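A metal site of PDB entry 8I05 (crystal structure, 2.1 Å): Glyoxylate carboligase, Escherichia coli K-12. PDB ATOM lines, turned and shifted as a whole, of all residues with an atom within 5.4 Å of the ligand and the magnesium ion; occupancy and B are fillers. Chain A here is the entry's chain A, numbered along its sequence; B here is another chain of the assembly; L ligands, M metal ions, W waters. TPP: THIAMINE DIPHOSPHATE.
Of the 34 residues printed, 3 come within 4 Å of the magnesium ion.
Water W2 lies within hydrogen-bond range of an oxygen (O2B) of the ligand (2.8 Å), the backbone carbonyl oxygen (O) of Val 472 (2.9 Å) and the side-chain amide nitrogen (ND2) of Asn 474 (3.3 Å).
Water W4 lies within hydrogen-bond range of O1A of the ligand (2.6 Å), O of Ile 394 (2.7 Å), OG of Ser 397 (2.7 Å) and N of Gly 446 (2.8 Å).
Water W3 lies within hydrogen-bond range of an oxygen (O2B) of the ligand and the side-chain amide nitrogen (ND2) of Asn 474.
Water W1 lies within hydrogen-bond range of the backbone carbonyl oxygen of Val 26 of chain B (2.8 Å), the backbone NH of Thr 76 of chain B (2.9 Å) and a nitrogen (N1') of the ligand (3.2 Å).
CG2 of Ile 394 touches N4' of the ligand, 3.8 Å away.
Gly 395 touches the ligand (CA to O3B, 3.5 Å).
CA of Gly 446 touches O1A of the ligand (3.6 Å).
CE2 of Phe 452 touches CM2 of the ligand, at 3.8 Å.
CA of Leu 477 touches O7 of the ligand (3.7 Å).
CG1 of Ile 480 touches CM4 of the ligand (3.6 Å).
CG1 of Val 26 of chain B touches CM4 of the ligand, at 3.9 Å.
Pro 27 of chain B touches the ligand (O to CM4, 3.3 Å).
CG2 of Val 52 of chain B touches N1' of the ligand, 3.6 Å away.
Thr 76 of chain B touches the ligand (CG2 to C6', 3.7 Å).
Pro 79 of chain B touches the ligand (CG to N3', 3.7 Å).
OD2 of Asp 83 of chain B touches CM2 of the ligand, at 3.3 Å.
Hydrophobic or aromatic side chains that line the ligand: Ile 394, Leu 396, Leu 422, Phe 448, Phe 452, Leu 477, Leu 479, Ile 480, Val 26 of chain B, Val 52 of chain B and Pro 79 of chain B.
The side-chain carboxylate (OD2) of Asp 447 lies within hydrogen-bond range of the backbone NH (N) of Ala 475, at 3.2 Å.
The side-chain amide nitrogen (NE2) of Gln 116 of chain B sits at hydrogen-bond distance from the backbone carbonyl oxygen (O) of Ala 419, 2.7 Å away.
OG of Ser 445 lies within hydrogen-bond range of OD2 of Asp 449 (2.6 Å).
The side-chain carboxylate (OD2) of Asp 447 sits close to the side-chain amide oxygen (OD1) of Asn 473, 3.2 Å away.
The backbone carbonyl oxygen of Gly 420 is in hydrogen-bond range of the side-chain amide nitrogen of Gln 116 of chain B (3.2 Å).
The side-chain hydroxyl (OG) of Ser 397 sits at hydrogen-bond distance from the backbone NH (N) of Gly 446 (3.3 Å).
OD1 of Asn 474 binds the magnesium ion (2.0 Å).
O2A of the ligand is bound to the magnesium ion (2.2 Å).
The side-chain carboxylate (OD1) of Asp 447 is bound to the magnesium ion.
O of Tyr 476 is bound to the magnesium ion.
The magnesium ion is bound by an oxygen (O1B) of the ligand.
Water W2 binds the magnesium ion (2.3 Å).
The backbone NH (N) of Leu 422 lies within hydrogen-bond range of a nitrogen (N3') of the ligand (3.5 Å).
N of Gly 478 sits at hydrogen-bond distance from O3B of the ligand (3.3 Å).
An oxygen (O3B) of the ligand lies within hydrogen-bond range of the backbone NH (N) of Leu 479 (2.9 Å).
N of Phe 448 sits close to O2A of the ligand, at 3.0 Å.
The backbone NH of Asp 449 sits at hydrogen-bond distance from an oxygen (O1A) of the ligand, 2.9 Å away.
NE2 of Gln 116 of chain B sits close to N4' of the ligand.
An oxygen (O2B) of the ligand lies within hydrogen-bond range of the backbone NH (N) of Ser 397 (3.0 Å).
O of Gly 420 sits at hydrogen-bond distance from N4' of the ligand (2.9 Å).
An oxygen (O2A) of the ligand sits close to the backbone NH (N) of Asp 447 (3.3 Å).
An oxygen (O3B) of the ligand lies within hydrogen-bond range of the backbone NH of Leu 396.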
ATOM      1  N   ILE A 394       9.407  26.835 -11.541  1.00  0.00           N
ATOM      2  CA  ILE A 394      10.255  26.511 -12.692  1.00  0.00           C
ATOM      3  C   ILE A 394      10.721  25.074 -12.550  1.00  0.00           C
ATOM      4  O   ILE A 394      10.700  24.501 -11.451  1.00  0.00           O
ATOM      5  CB  ILE A 394      11.458  27.491 -12.775  1.00  0.00           C
ATOM      6  CG1 ILE A 394      12.164  27.398 -14.128  1.00  0.00           C
ATOM      7  CG2 ILE A 394      12.434  27.263 -11.621  1.00  0.00           C
ATOM      8  CD1 ILE A 394      13.227  28.480 -14.316  1.00  0.00           C
ATOM      9  N   GLY A 395      11.196  24.493 -13.651  1.00  0.00           N
ATOM     10  CA  GLY A 395      11.579  23.098 -13.726  1.00  0.00           C
ATOM     11  C   GLY A 395      10.689  22.339 -14.690  1.00  0.00           C
ATOM     12  O   GLY A 395       9.673  22.832 -15.175  1.00  0.00           O
ATOM     13  N   LEU A 396      11.085  21.088 -14.939  1.00  0.00           N
ATOM     14  CA  LEU A 396      10.232  20.236 -15.758  1.00  0.00           C
ATOM     15  C   LEU A 396       8.851  20.081 -15.123  1.00  0.00           C
ATOM     16  O   LEU A 396       7.846  19.945 -15.817  1.00  0.00           O
ATOM     17  CB  LEU A 396      10.896  18.875 -15.970  1.00  0.00           C
ATOM     18  CG  LEU A 396      12.208  18.888 -16.765  1.00  0.00           C
ATOM     19  CD1 LEU A 396      12.716  17.467 -17.020  1.00  0.00           C
ATOM     20  CD2 LEU A 396      12.043  19.636 -18.060  1.00  0.00           C
ATOM     21  N   SER A 397       8.798  20.146 -13.794  1.00  0.00           N
ATOM     22  CA  SER A 397       7.537  20.144 -13.076  1.00  0.00           C
ATOM     23  C   SER A 397       6.628  21.236 -13.594  1.00  0.00           C
ATOM     24  O   SER A 397       5.459  20.992 -13.936  1.00  0.00           O
ATOM     25  CB  SER A 397       7.806  20.362 -11.590  1.00  0.00           C
ATOM     26  OG  SER A 397       8.658  21.516 -11.453  1.00  0.00           O
ATOM     27  N   ALA A 419      11.711  35.582 -13.737  1.00  0.00           N
ATOM     28  CA  ALA A 419      12.893  35.352 -12.905  1.00  0.00           C
ATOM     29  C   ALA A 419      13.035  33.903 -12.443  1.00  0.00           C
ATOM     30  O   ALA A 419      14.158  33.398 -12.362  1.00  0.00           O
ATOM     31  CB  ALA A 419      12.895  36.262 -11.677  1.00  0.00           C
ATOM     32  N   GLY A 420      11.928  33.231 -12.111  1.00  0.00           N
ATOM     33  CA  GLY A 420      11.958  31.837 -11.759  1.00  0.00           C
ATOM     34  C   GLY A 420      12.893  31.411 -10.634  1.00  0.00           C
ATOM     35  O   GLY A 420      13.648  30.449 -10.791  1.00  0.00           O
ATOM     36  N   PRO A 421      12.884  32.096  -9.483  1.00  0.00           N
ATOM     37  CA  PRO A 421      13.786  31.680  -8.380  1.00  0.00           C
ATOM     38  C   PRO A 421      13.290  30.424  -7.694  1.00  0.00           C
ATOM     39  O   PRO A 421      12.162  30.374  -7.191  1.00  0.00           O
ATOM     40  CB  PRO A 421      13.740  32.867  -7.422  1.00  0.00           C
ATOM     41  CG  PRO A 421      12.417  33.507  -7.691  1.00  0.00           C
ATOM     42  CD  PRO A 421      12.124  33.306  -9.159  1.00  0.00           C
ATOM     43  N   LEU A 422      14.162  29.418  -7.593  1.00  0.00           N
ATOM     44  CA  LEU A 422      13.831  28.206  -6.858  1.00  0.00           C
ATOM     45  C   LEU A 422      13.518  28.559  -5.414  1.00  0.00           C
ATOM     46  O   LEU A 422      14.146  29.449  -4.848  1.00  0.00           O
ATOM     47  CB  LEU A 422      14.988  27.197  -6.934  1.00  0.00           C
ATOM     48  CG  LEU A 422      15.201  26.575  -8.325  1.00  0.00           C
ATOM     49  CD1 LEU A 422      16.529  25.786  -8.431  1.00  0.00           C
ATOM     50  CD2 LEU A 422      14.004  25.671  -8.682  1.00  0.00           C
ATOM     51  N   SER A 445       5.578  21.723  -7.340  1.00  0.00           N
ATOM     52  CA  SER A 445       7.025  21.834  -7.293  1.00  0.00           C
ATOM     53  C   SER A 445       7.660  20.537  -7.739  1.00  0.00           C
ATOM     54  O   SER A 445       7.070  19.449  -7.553  1.00  0.00           O
ATOM     55  CB  SER A 445       7.575  22.115  -5.869  1.00  0.00           C
ATOM     56  OG  SER A 445       7.165  23.357  -5.340  1.00  0.00           O
ATOM     57  N   GLY A 446       8.890  20.635  -8.286  1.00  0.00           N
ATOM     58  CA  GLY A 446       9.826  19.528  -8.259  1.00  0.00           C
ATOM     59  C   GLY A 446      10.524  19.424  -6.895  1.00  0.00           C
ATOM     60  O   GLY A 446      10.347  20.264  -6.020  1.00  0.00           O
ATOM     61  N   ASP A 447      11.319  18.357  -6.725  1.00  0.00           N
ATOM     62  CA  ASP A 447      11.945  18.135  -5.421  1.00  0.00           C
ATOM     63  C   ASP A 447      12.976  19.220  -5.078  1.00  0.00           C
ATOM     64  O   ASP A 447      13.043  19.660  -3.928  1.00  0.00           O
ATOM     65  CB  ASP A 447      12.560  16.730  -5.334  1.00  0.00           C
ATOM     66  CG  ASP A 447      13.283  16.300  -6.597  1.00  0.00           C
ATOM     67  OD1 ASP A 447      12.761  16.535  -7.723  1.00  0.00           O
ATOM     68  OD2 ASP A 447      14.376  15.715  -6.466  1.00  0.00           O
ATOM     69  N   PHE A 448      13.720  19.724  -6.060  1.00  0.00           N
ATOM     70  CA  PHE A 448      14.758  20.719  -5.778  1.00  0.00           C
ATOM     71  C   PHE A 448      14.120  22.045  -5.377  1.00  0.00           C
ATOM     72  O   PHE A 448      14.450  22.597  -4.320  1.00  0.00           O
ATOM     73  CB  PHE A 448      15.662  20.892  -7.009  1.00  0.00           C
ATOM     74  CG  PHE A 448      17.038  21.476  -6.710  1.00  0.00           C
ATOM     75  CD1 PHE A 448      17.860  20.934  -5.708  1.00  0.00           C
ATOM     76  CD2 PHE A 448      17.543  22.498  -7.494  1.00  0.00           C
ATOM     77  CE1 PHE A 448      19.127  21.438  -5.471  1.00  0.00           C
ATOM     78  CE2 PHE A 448      18.806  23.011  -7.260  1.00  0.00           C
ATOM     79  CZ  PHE A 448      19.621  22.474  -6.237  1.00  0.00           C
ATOM     80  N   ASP A 449      13.158  22.532  -6.174  1.00  0.00           N
ATOM     81  CA  ASP A 449      12.384  23.710  -5.790  1.00  0.00           C
ATOM     82  C   ASP A 449      11.827  23.558  -4.381  1.00  0.00           C
ATOM     83  O   ASP A 449      11.920  24.472  -3.551  1.00  0.00           O
ATOM     84  CB  ASP A 449      11.247  23.946  -6.796  1.00  0.00           C
ATOM     85  CG  ASP A 449      10.248  25.047  -6.373  1.00  0.00           C
ATOM     86  OD1 ASP A 449      10.655  26.146  -5.926  1.00  0.00           O
ATOM     87  OD2 ASP A 449       9.028  24.826  -6.520  1.00  0.00           O
ATOM     88  N   PHE A 450      11.254  22.382  -4.104  1.00  0.00           N
ATOM     89  CA  PHE A 450      10.616  22.178  -2.815  1.00  0.00           C
ATOM     90  C   PHE A 450      11.610  22.271  -1.650  1.00  0.00           C
ATOM     91  O   PHE A 450      11.267  22.755  -0.578  1.00  0.00           O
ATOM     92  CB  PHE A 450       9.909  20.815  -2.824  1.00  0.00           C
ATOM     93  CG  PHE A 450       8.972  20.583  -1.673  1.00  0.00           C
ATOM     94  CD1 PHE A 450       7.751  21.207  -1.618  1.00  0.00           C
ATOM     95  CD2 PHE A 450       9.310  19.684  -0.674  1.00  0.00           C
ATOM     96  CE1 PHE A 450       6.893  20.955  -0.567  1.00  0.00           C
ATOM     97  CE2 PHE A 450       8.438  19.437   0.377  1.00  0.00           C
ATOM     98  CZ  PHE A 450       7.250  20.067   0.436  1.00  0.00           C
ATOM     99  N   PHE A 452      14.507  24.169  -1.422  1.00  0.00           N
ATOM    100  CA  PHE A 452      15.178  25.459  -1.179  1.00  0.00           C
ATOM    101  C   PHE A 452      14.663  26.148   0.078  1.00  0.00           C
ATOM    102  O   PHE A 452      15.447  26.565   0.940  1.00  0.00           O
ATOM    103  CB  PHE A 452      14.989  26.396  -2.378  1.00  0.00           C
ATOM    104  CG  PHE A 452      16.145  26.439  -3.353  1.00  0.00           C
ATOM    105  CD1 PHE A 452      16.606  25.288  -3.962  1.00  0.00           C
ATOM    106  CD2 PHE A 452      16.727  27.651  -3.702  1.00  0.00           C
ATOM    107  CE1 PHE A 452      17.655  25.332  -4.880  1.00  0.00           C
ATOM    108  CE2 PHE A 452      17.763  27.700  -4.621  1.00  0.00           C
ATOM    109  CZ  PHE A 452      18.225  26.537  -5.202  1.00  0.00           C
ATOM    110  N   VAL A 472       6.444  16.563  -7.214  1.00  0.00           N
ATOM    111  CA  VAL A 472       6.768  15.519  -8.171  1.00  0.00           C
ATOM    112  C   VAL A 472       8.276  15.287  -8.081  1.00  0.00           C
ATOM    113  O   VAL A 472       9.076  16.173  -8.403  1.00  0.00           O
ATOM    114  CB  VAL A 472       6.275  15.849  -9.594  1.00  0.00           C
ATOM    115  CG1 VAL A 472       4.754  15.910  -9.618  1.00  0.00           C
ATOM    116  CG2 VAL A 472       6.792  17.180 -10.108  1.00  0.00           C
ATOM    117  N   ASN A 473       8.657  14.102  -7.622  1.00  0.00           N
ATOM    118  CA  ASN A 473      10.019  13.836  -7.137  1.00  0.00           C
ATOM    119  C   ASN A 473      10.716  12.886  -8.104  1.00  0.00           C
ATOM    120  O   ASN A 473      10.377  11.699  -8.181  1.00  0.00           O
ATOM    121  CB  ASN A 473       9.952  13.251  -5.720  1.00  0.00           C
ATOM    122  CG  ASN A 473      11.344  12.933  -5.128  1.00  0.00           C
ATOM    123  OD1 ASN A 473      12.373  13.283  -5.705  1.00  0.00           O
ATOM    124  ND2 ASN A 473      11.368  12.259  -3.980  1.00  0.00           N
ATOM    125  N   ASN A 474      11.696  13.399  -8.846  1.00  0.00           N
ATOM    126  CA  ASN A 474      12.547  12.555  -9.681  1.00  0.00           C
ATOM    127  C   ASN A 474      13.980  12.406  -9.135  1.00  0.00           C
ATOM    128  O   ASN A 474      14.825  11.827  -9.821  1.00  0.00           O
ATOM    129  CB  ASN A 474      12.564  13.085 -11.111  1.00  0.00           C
ATOM    130  CG  ASN A 474      12.895  14.584 -11.203  1.00  0.00           C
ATOM    131  OD1 ASN A 474      13.436  15.170 -10.252  1.00  0.00           O
ATOM    132  ND2 ASN A 474      12.572  15.201 -12.344  1.00  0.00           N
ATOM    133  N   ALA A 475      14.268  12.919  -7.934  1.00  0.00           N
ATOM    134  CA  ALA A 475      15.632  12.955  -7.372  1.00  0.00           C
ATOM    135  C   ALA A 475      16.647  13.561  -8.356  1.00  0.00           C
ATOM    136  O   ALA A 475      17.807  13.145  -8.406  1.00  0.00           O
ATOM    137  CB  ALA A 475      16.083  11.569  -6.910  1.00  0.00           C
ATOM    138  N   TYR A 476      16.227  14.570  -9.107  1.00  0.00           N
ATOM    139  CA  TYR A 476      17.054  15.192 -10.140  1.00  0.00           C
ATOM    140  C   TYR A 476      16.769  16.680 -10.172  1.00  0.00           C
ATOM    141  O   TYR A 476      15.663  17.108  -9.849  1.00  0.00           O
ATOM    142  CB  TYR A 476      16.726  14.633 -11.535  1.00  0.00           C
ATOM    143  CG  TYR A 476      17.681  13.676 -12.213  1.00  0.00           C
ATOM    144  CD1 TYR A 476      18.840  14.133 -12.810  1.00  0.00           C
ATOM    145  CD2 TYR A 476      17.375  12.328 -12.322  1.00  0.00           C
ATOM    146  CE1 TYR A 476      19.688  13.255 -13.476  1.00  0.00           C
ATOM    147  CE2 TYR A 476      18.220  11.441 -12.974  1.00  0.00           C
ATOM    148  CZ  TYR A 476      19.376  11.916 -13.555  1.00  0.00           C
ATOM    149  OH  TYR A 476      20.231  11.058 -14.209  1.00  0.00           O
ATOM    150  N   LEU A 477      17.761  17.482 -10.602  1.00  0.00           N
ATOM    151  CA  LEU A 477      17.459  18.790 -11.190  1.00  0.00           C
ATOM    152  C   LEU A 477      17.079  18.516 -12.638  1.00  0.00           C
ATOM    153  O   LEU A 477      17.917  18.539 -13.543  1.00  0.00           O
ATOM    154  CB  LEU A 477      18.649  19.749 -11.120  1.00  0.00           C
ATOM    155  CG  LEU A 477      19.639  19.851  -9.959  1.00  0.00           C
ATOM    156  CD1 LEU A 477      20.345  21.210  -9.959  1.00  0.00           C
ATOM    157  CD2 LEU A 477      19.019  19.555  -8.622  1.00  0.00           C
ATOM    158  N   GLY A 478      15.791  18.205 -12.870  1.00  0.00           N
ATOM    159  CA  GLY A 478      15.411  17.599 -14.128  1.00  0.00           C
ATOM    160  C   GLY A 478      15.576  18.516 -15.329  1.00  0.00           C
ATOM    161  O   GLY A 478      16.079  18.101 -16.375  1.00  0.00           O
ATOM    162  N   LEU A 479      15.197  19.784 -15.188  1.00  0.00           N
ATOM    163  CA  LEU A 479      15.372  20.716 -16.298  1.00  0.00           C
ATOM    164  C   LEU A 479      16.851  20.856 -16.663  1.00  0.00           C
ATOM    165  O   LEU A 479      17.163  21.001 -17.852  1.00  0.00           O
ATOM    166  CB  LEU A 479      14.780  22.081 -15.953  1.00  0.00           C
ATOM    167  CG  LEU A 479      14.806  23.164 -17.055  1.00  0.00           C
ATOM    168  CD1 LEU A 479      14.282  22.612 -18.385  1.00  0.00           C
ATOM    169  CD2 LEU A 479      14.027  24.416 -16.627  1.00  0.00           C
ATOM    170  N   ILE A 480      17.762  20.763 -15.693  1.00  0.00           N
ATOM    171  CA  ILE A 480      19.183  20.976 -16.006  1.00  0.00           C
ATOM    172  C   ILE A 480      19.788  19.727 -16.601  1.00  0.00           C
ATOM    173  O   ILE A 480      20.653  19.806 -17.489  1.00  0.00           O
ATOM    174  CB  ILE A 480      19.976  21.453 -14.775  1.00  0.00           C
ATOM    175  CG1 ILE A 480      19.241  22.623 -14.085  1.00  0.00           C
ATOM    176  CG2 ILE A 480      21.408  21.874 -15.180  1.00  0.00           C
ATOM    177  CD1 ILE A 480      18.756  23.722 -15.043  1.00  0.00           C
ATOM    178  N   LEU A 495      20.150  14.205  -7.084  1.00  0.00           N
ATOM    179  CA  LEU A 495      19.916  14.403  -5.659  1.00  0.00           C
ATOM    180  C   LEU A 495      19.757  13.087  -4.899  1.00  0.00           C
ATOM    181  O   LEU A 495      19.575  13.119  -3.672  1.00  0.00           O
ATOM    182  CB  LEU A 495      18.685  15.280  -5.450  1.00  0.00           C
ATOM    183  CG  LEU A 495      18.798  16.692  -6.047  1.00  0.00           C
ATOM    184  CD1 LEU A 495      17.439  17.340  -6.085  1.00  0.00           C
ATOM    185  CD2 LEU A 495      19.787  17.564  -5.233  1.00  0.00           C
ATOM    186  N   VAL B  26      25.203  25.269  -7.821  1.00  0.00           N
ATOM    187  CA  VAL B  26      23.936  24.779  -8.339  1.00  0.00           C
ATOM    188  C   VAL B  26      23.967  25.051  -9.846  1.00  0.00           C
ATOM    189  O   VAL B  26      23.993  26.221 -10.239  1.00  0.00           O
ATOM    190  CB  VAL B  26      22.734  25.468  -7.690  1.00  0.00           C
ATOM    191  CG1 VAL B  26      21.392  25.007  -8.343  1.00  0.00           C
ATOM    192  CG2 VAL B  26      22.716  25.252  -6.176  1.00  0.00           C
ATOM    193  N   PRO B  27      24.010  24.031 -10.702  1.00  0.00           N
ATOM    194  CA  PRO B  27      24.073  24.272 -12.144  1.00  0.00           C
ATOM    195  C   PRO B  27      22.747  24.799 -12.682  1.00  0.00           C
ATOM    196  O   PRO B  27      21.691  24.711 -12.029  1.00  0.00           O
ATOM    197  CB  PRO B  27      24.387  22.888 -12.731  1.00  0.00           C
ATOM    198  CG  PRO B  27      23.841  21.956 -11.740  1.00  0.00           C
ATOM    199  CD  PRO B  27      24.036  22.580 -10.401  1.00  0.00           C
ATOM    200  N   GLY B  28      22.826  25.377 -13.878  1.00  0.00           N
ATOM    201  CA  GLY B  28      21.657  25.794 -14.639  1.00  0.00           C
ATOM    202  C   GLY B  28      22.075  25.959 -16.081  1.00  0.00           C
ATOM    203  O   GLY B  28      23.260  25.914 -16.407  1.00  0.00           O
ATOM    204  N   VAL B  52      21.050  28.112  -3.484  1.00  0.00           N
ATOM    205  CA  VAL B  52      22.233  28.837  -3.937  1.00  0.00           C
ATOM    206  C   VAL B  52      22.847  29.602  -2.766  1.00  0.00           C
ATOM    207  O   VAL B  52      24.077  29.721  -2.685  1.00  0.00           O
ATOM    208  CB  VAL B  52      21.886  29.754  -5.129  1.00  0.00           C
ATOM    209  CG1 VAL B  52      23.039  30.746  -5.398  1.00  0.00           C
ATOM    210  CG2 VAL B  52      21.643  28.907  -6.366  1.00  0.00           C
ATOM    211  N   THR B  76      23.822  29.772 -11.890  1.00  0.00           N
ATOM    212  CA  THR B  76      23.334  30.125 -13.225  1.00  0.00           C
ATOM    213  C   THR B  76      23.000  31.624 -13.256  1.00  0.00           C
ATOM    214  O   THR B  76      23.349  32.381 -12.345  1.00  0.00           O
ATOM    215  CB  THR B  76      22.143  29.217 -13.603  1.00  0.00           C
ATOM    216  OG1 THR B  76      21.921  29.278 -15.007  1.00  0.00           O
ATOM    217  CG2 THR B  76      20.859  29.624 -12.896  1.00  0.00           C
ATOM    218  N   PRO B  79      18.242  34.605 -10.859  1.00  0.00           N
ATOM    219  CA  PRO B  79      18.110  34.547  -9.401  1.00  0.00           C
ATOM    220  C   PRO B  79      19.270  33.873  -8.679  1.00  0.00           C
ATOM    221  O   PRO B  79      19.382  34.028  -7.465  1.00  0.00           O
ATOM    222  CB  PRO B  79      16.793  33.786  -9.179  1.00  0.00           C
ATOM    223  CG  PRO B  79      16.689  32.927 -10.384  1.00  0.00           C
ATOM    224  CD  PRO B  79      17.262  33.731 -11.531  1.00  0.00           C
ATOM    225  N   ALA B  80      20.094  33.074  -9.355  1.00  0.00           N
ATOM    226  CA  ALA B  80      21.258  32.531  -8.670  1.00  0.00           C
ATOM    227  C   ALA B  80      22.191  33.650  -8.198  1.00  0.00           C
ATOM    228  O   ALA B  80      22.596  33.675  -7.040  1.00  0.00           O
ATOM    229  CB  ALA B  80      22.008  31.546  -9.584  1.00  0.00           C
ATOM    230  N   ASP B  83      20.763  35.489  -5.265  1.00  0.00           N
ATOM    231  CA  ASP B  83      20.864  34.659  -4.070  1.00  0.00           C
ATOM    232  C   ASP B  83      22.278  34.651  -3.473  1.00  0.00           C
ATOM    233  O   ASP B  83      22.453  34.079  -2.388  1.00  0.00           O
ATOM    234  CB  ASP B  83      20.478  33.219  -4.381  1.00  0.00           C
ATOM    235  CG  ASP B  83      18.953  32.981  -4.373  1.00  0.00           C
ATOM    236  OD1 ASP B  83      18.137  33.879  -3.983  1.00  0.00           O
ATOM    237  OD2 ASP B  83      18.608  31.849  -4.770  1.00  0.00           O
ATOM    238  N   GLN B 116      15.439  35.140 -17.312  1.00  0.00           N
ATOM    239  CA  GLN B 116      16.367  34.984 -16.184  1.00  0.00           C
ATOM    240  C   GLN B 116      17.700  35.712 -16.393  1.00  0.00           C
ATOM    241  O   GLN B 116      18.764  35.164 -16.121  1.00  0.00           O
ATOM    242  CB  GLN B 116      16.630  33.503 -15.878  1.00  0.00           C
ATOM    243  CG  GLN B 116      15.473  32.739 -15.280  1.00  0.00           C
ATOM    244  CD  GLN B 116      15.882  31.424 -14.602  1.00  0.00           C
ATOM    245  OE1 GLN B 116      16.632  30.617 -15.166  1.00  0.00           O
ATOM    246  NE2 GLN B 116      15.380  31.217 -13.384  1.00  0.00           N
HETATM  247  N1' TPP L   1      19.210  28.522  -9.058  1.00  0.00           N
HETATM  248  C2' TPP L   1      18.122  29.260  -8.784  1.00  0.00           C
HETATM  249  CM2 TPP L   1      18.144  30.062  -7.523  1.00  0.00           C
HETATM  250  N3' TPP L   1      17.034  29.362  -9.550  1.00  0.00           N
HETATM  251  C4' TPP L   1      17.002  28.650 -10.685  1.00  0.00           C
HETATM  252  N4' TPP L   1      15.889  28.749 -11.425  1.00  0.00           N
HETATM  253  C5' TPP L   1      18.083  27.799 -11.063  1.00  0.00           C
HETATM  254  C6' TPP L   1      19.161  27.803 -10.188  1.00  0.00           C
HETATM  255  C7' TPP L   1      18.122  26.977 -12.334  1.00  0.00           C
HETATM  256  N3  TPP L   1      17.124  25.884 -12.392  1.00  0.00           N
HETATM  257  C2  TPP L   1      15.982  25.972 -13.057  1.00  0.00           C
HETATM  258  S1  TPP L   1      15.058  24.560 -12.962  1.00  0.00           S
HETATM  259  C5  TPP L   1      16.289  23.791 -12.022  1.00  0.00           C
HETATM  260  C4  TPP L   1      17.336  24.643 -11.788  1.00  0.00           C
HETATM  261  CM4 TPP L   1      18.578  24.365 -11.008  1.00  0.00           C
HETATM  262  C6  TPP L   1      16.060  22.402 -11.519  1.00  0.00           C
HETATM  263  C7  TPP L   1      14.743  22.288 -10.800  1.00  0.00           C
HETATM  264  O7  TPP L   1      14.549  20.927 -10.368  1.00  0.00           O
HETATM  265  PA  TPP L   1      13.249  20.423  -9.635  1.00  0.00           P
HETATM  266  O1A TPP L   1      12.650  21.602  -8.889  1.00  0.00           O
HETATM  267  O2A TPP L   1      13.560  19.127  -8.998  1.00  0.00           O
HETATM  268  O3A TPP L   1      12.410  20.146 -10.936  1.00  0.00           O
HETATM  269  PB  TPP L   1      12.449  19.124 -12.142  1.00  0.00           P
HETATM  270  O1B TPP L   1      13.367  17.999 -11.787  1.00  0.00           O
HETATM  271  O2B TPP L   1      10.974  18.713 -12.351  1.00  0.00           O
HETATM  272  O3B TPP L   1      12.988  19.934 -13.321  1.00  0.00           O
HETATM  273 MG    MG M   1      13.482  17.086  -9.689  1.00  0.00          MG
HETATM  274  O   HOH W   1      22.253  28.324  -9.855  1.00  0.00           O
HETATM  275  O   HOH W   2      11.177  17.107 -10.104  1.00  0.00           O
HETATM  276  O   HOH W   3       9.458  16.467 -13.258  1.00  0.00           O
HETATM  277  O   HOH W   4      10.311  22.615  -9.613  1.00  0.00           O
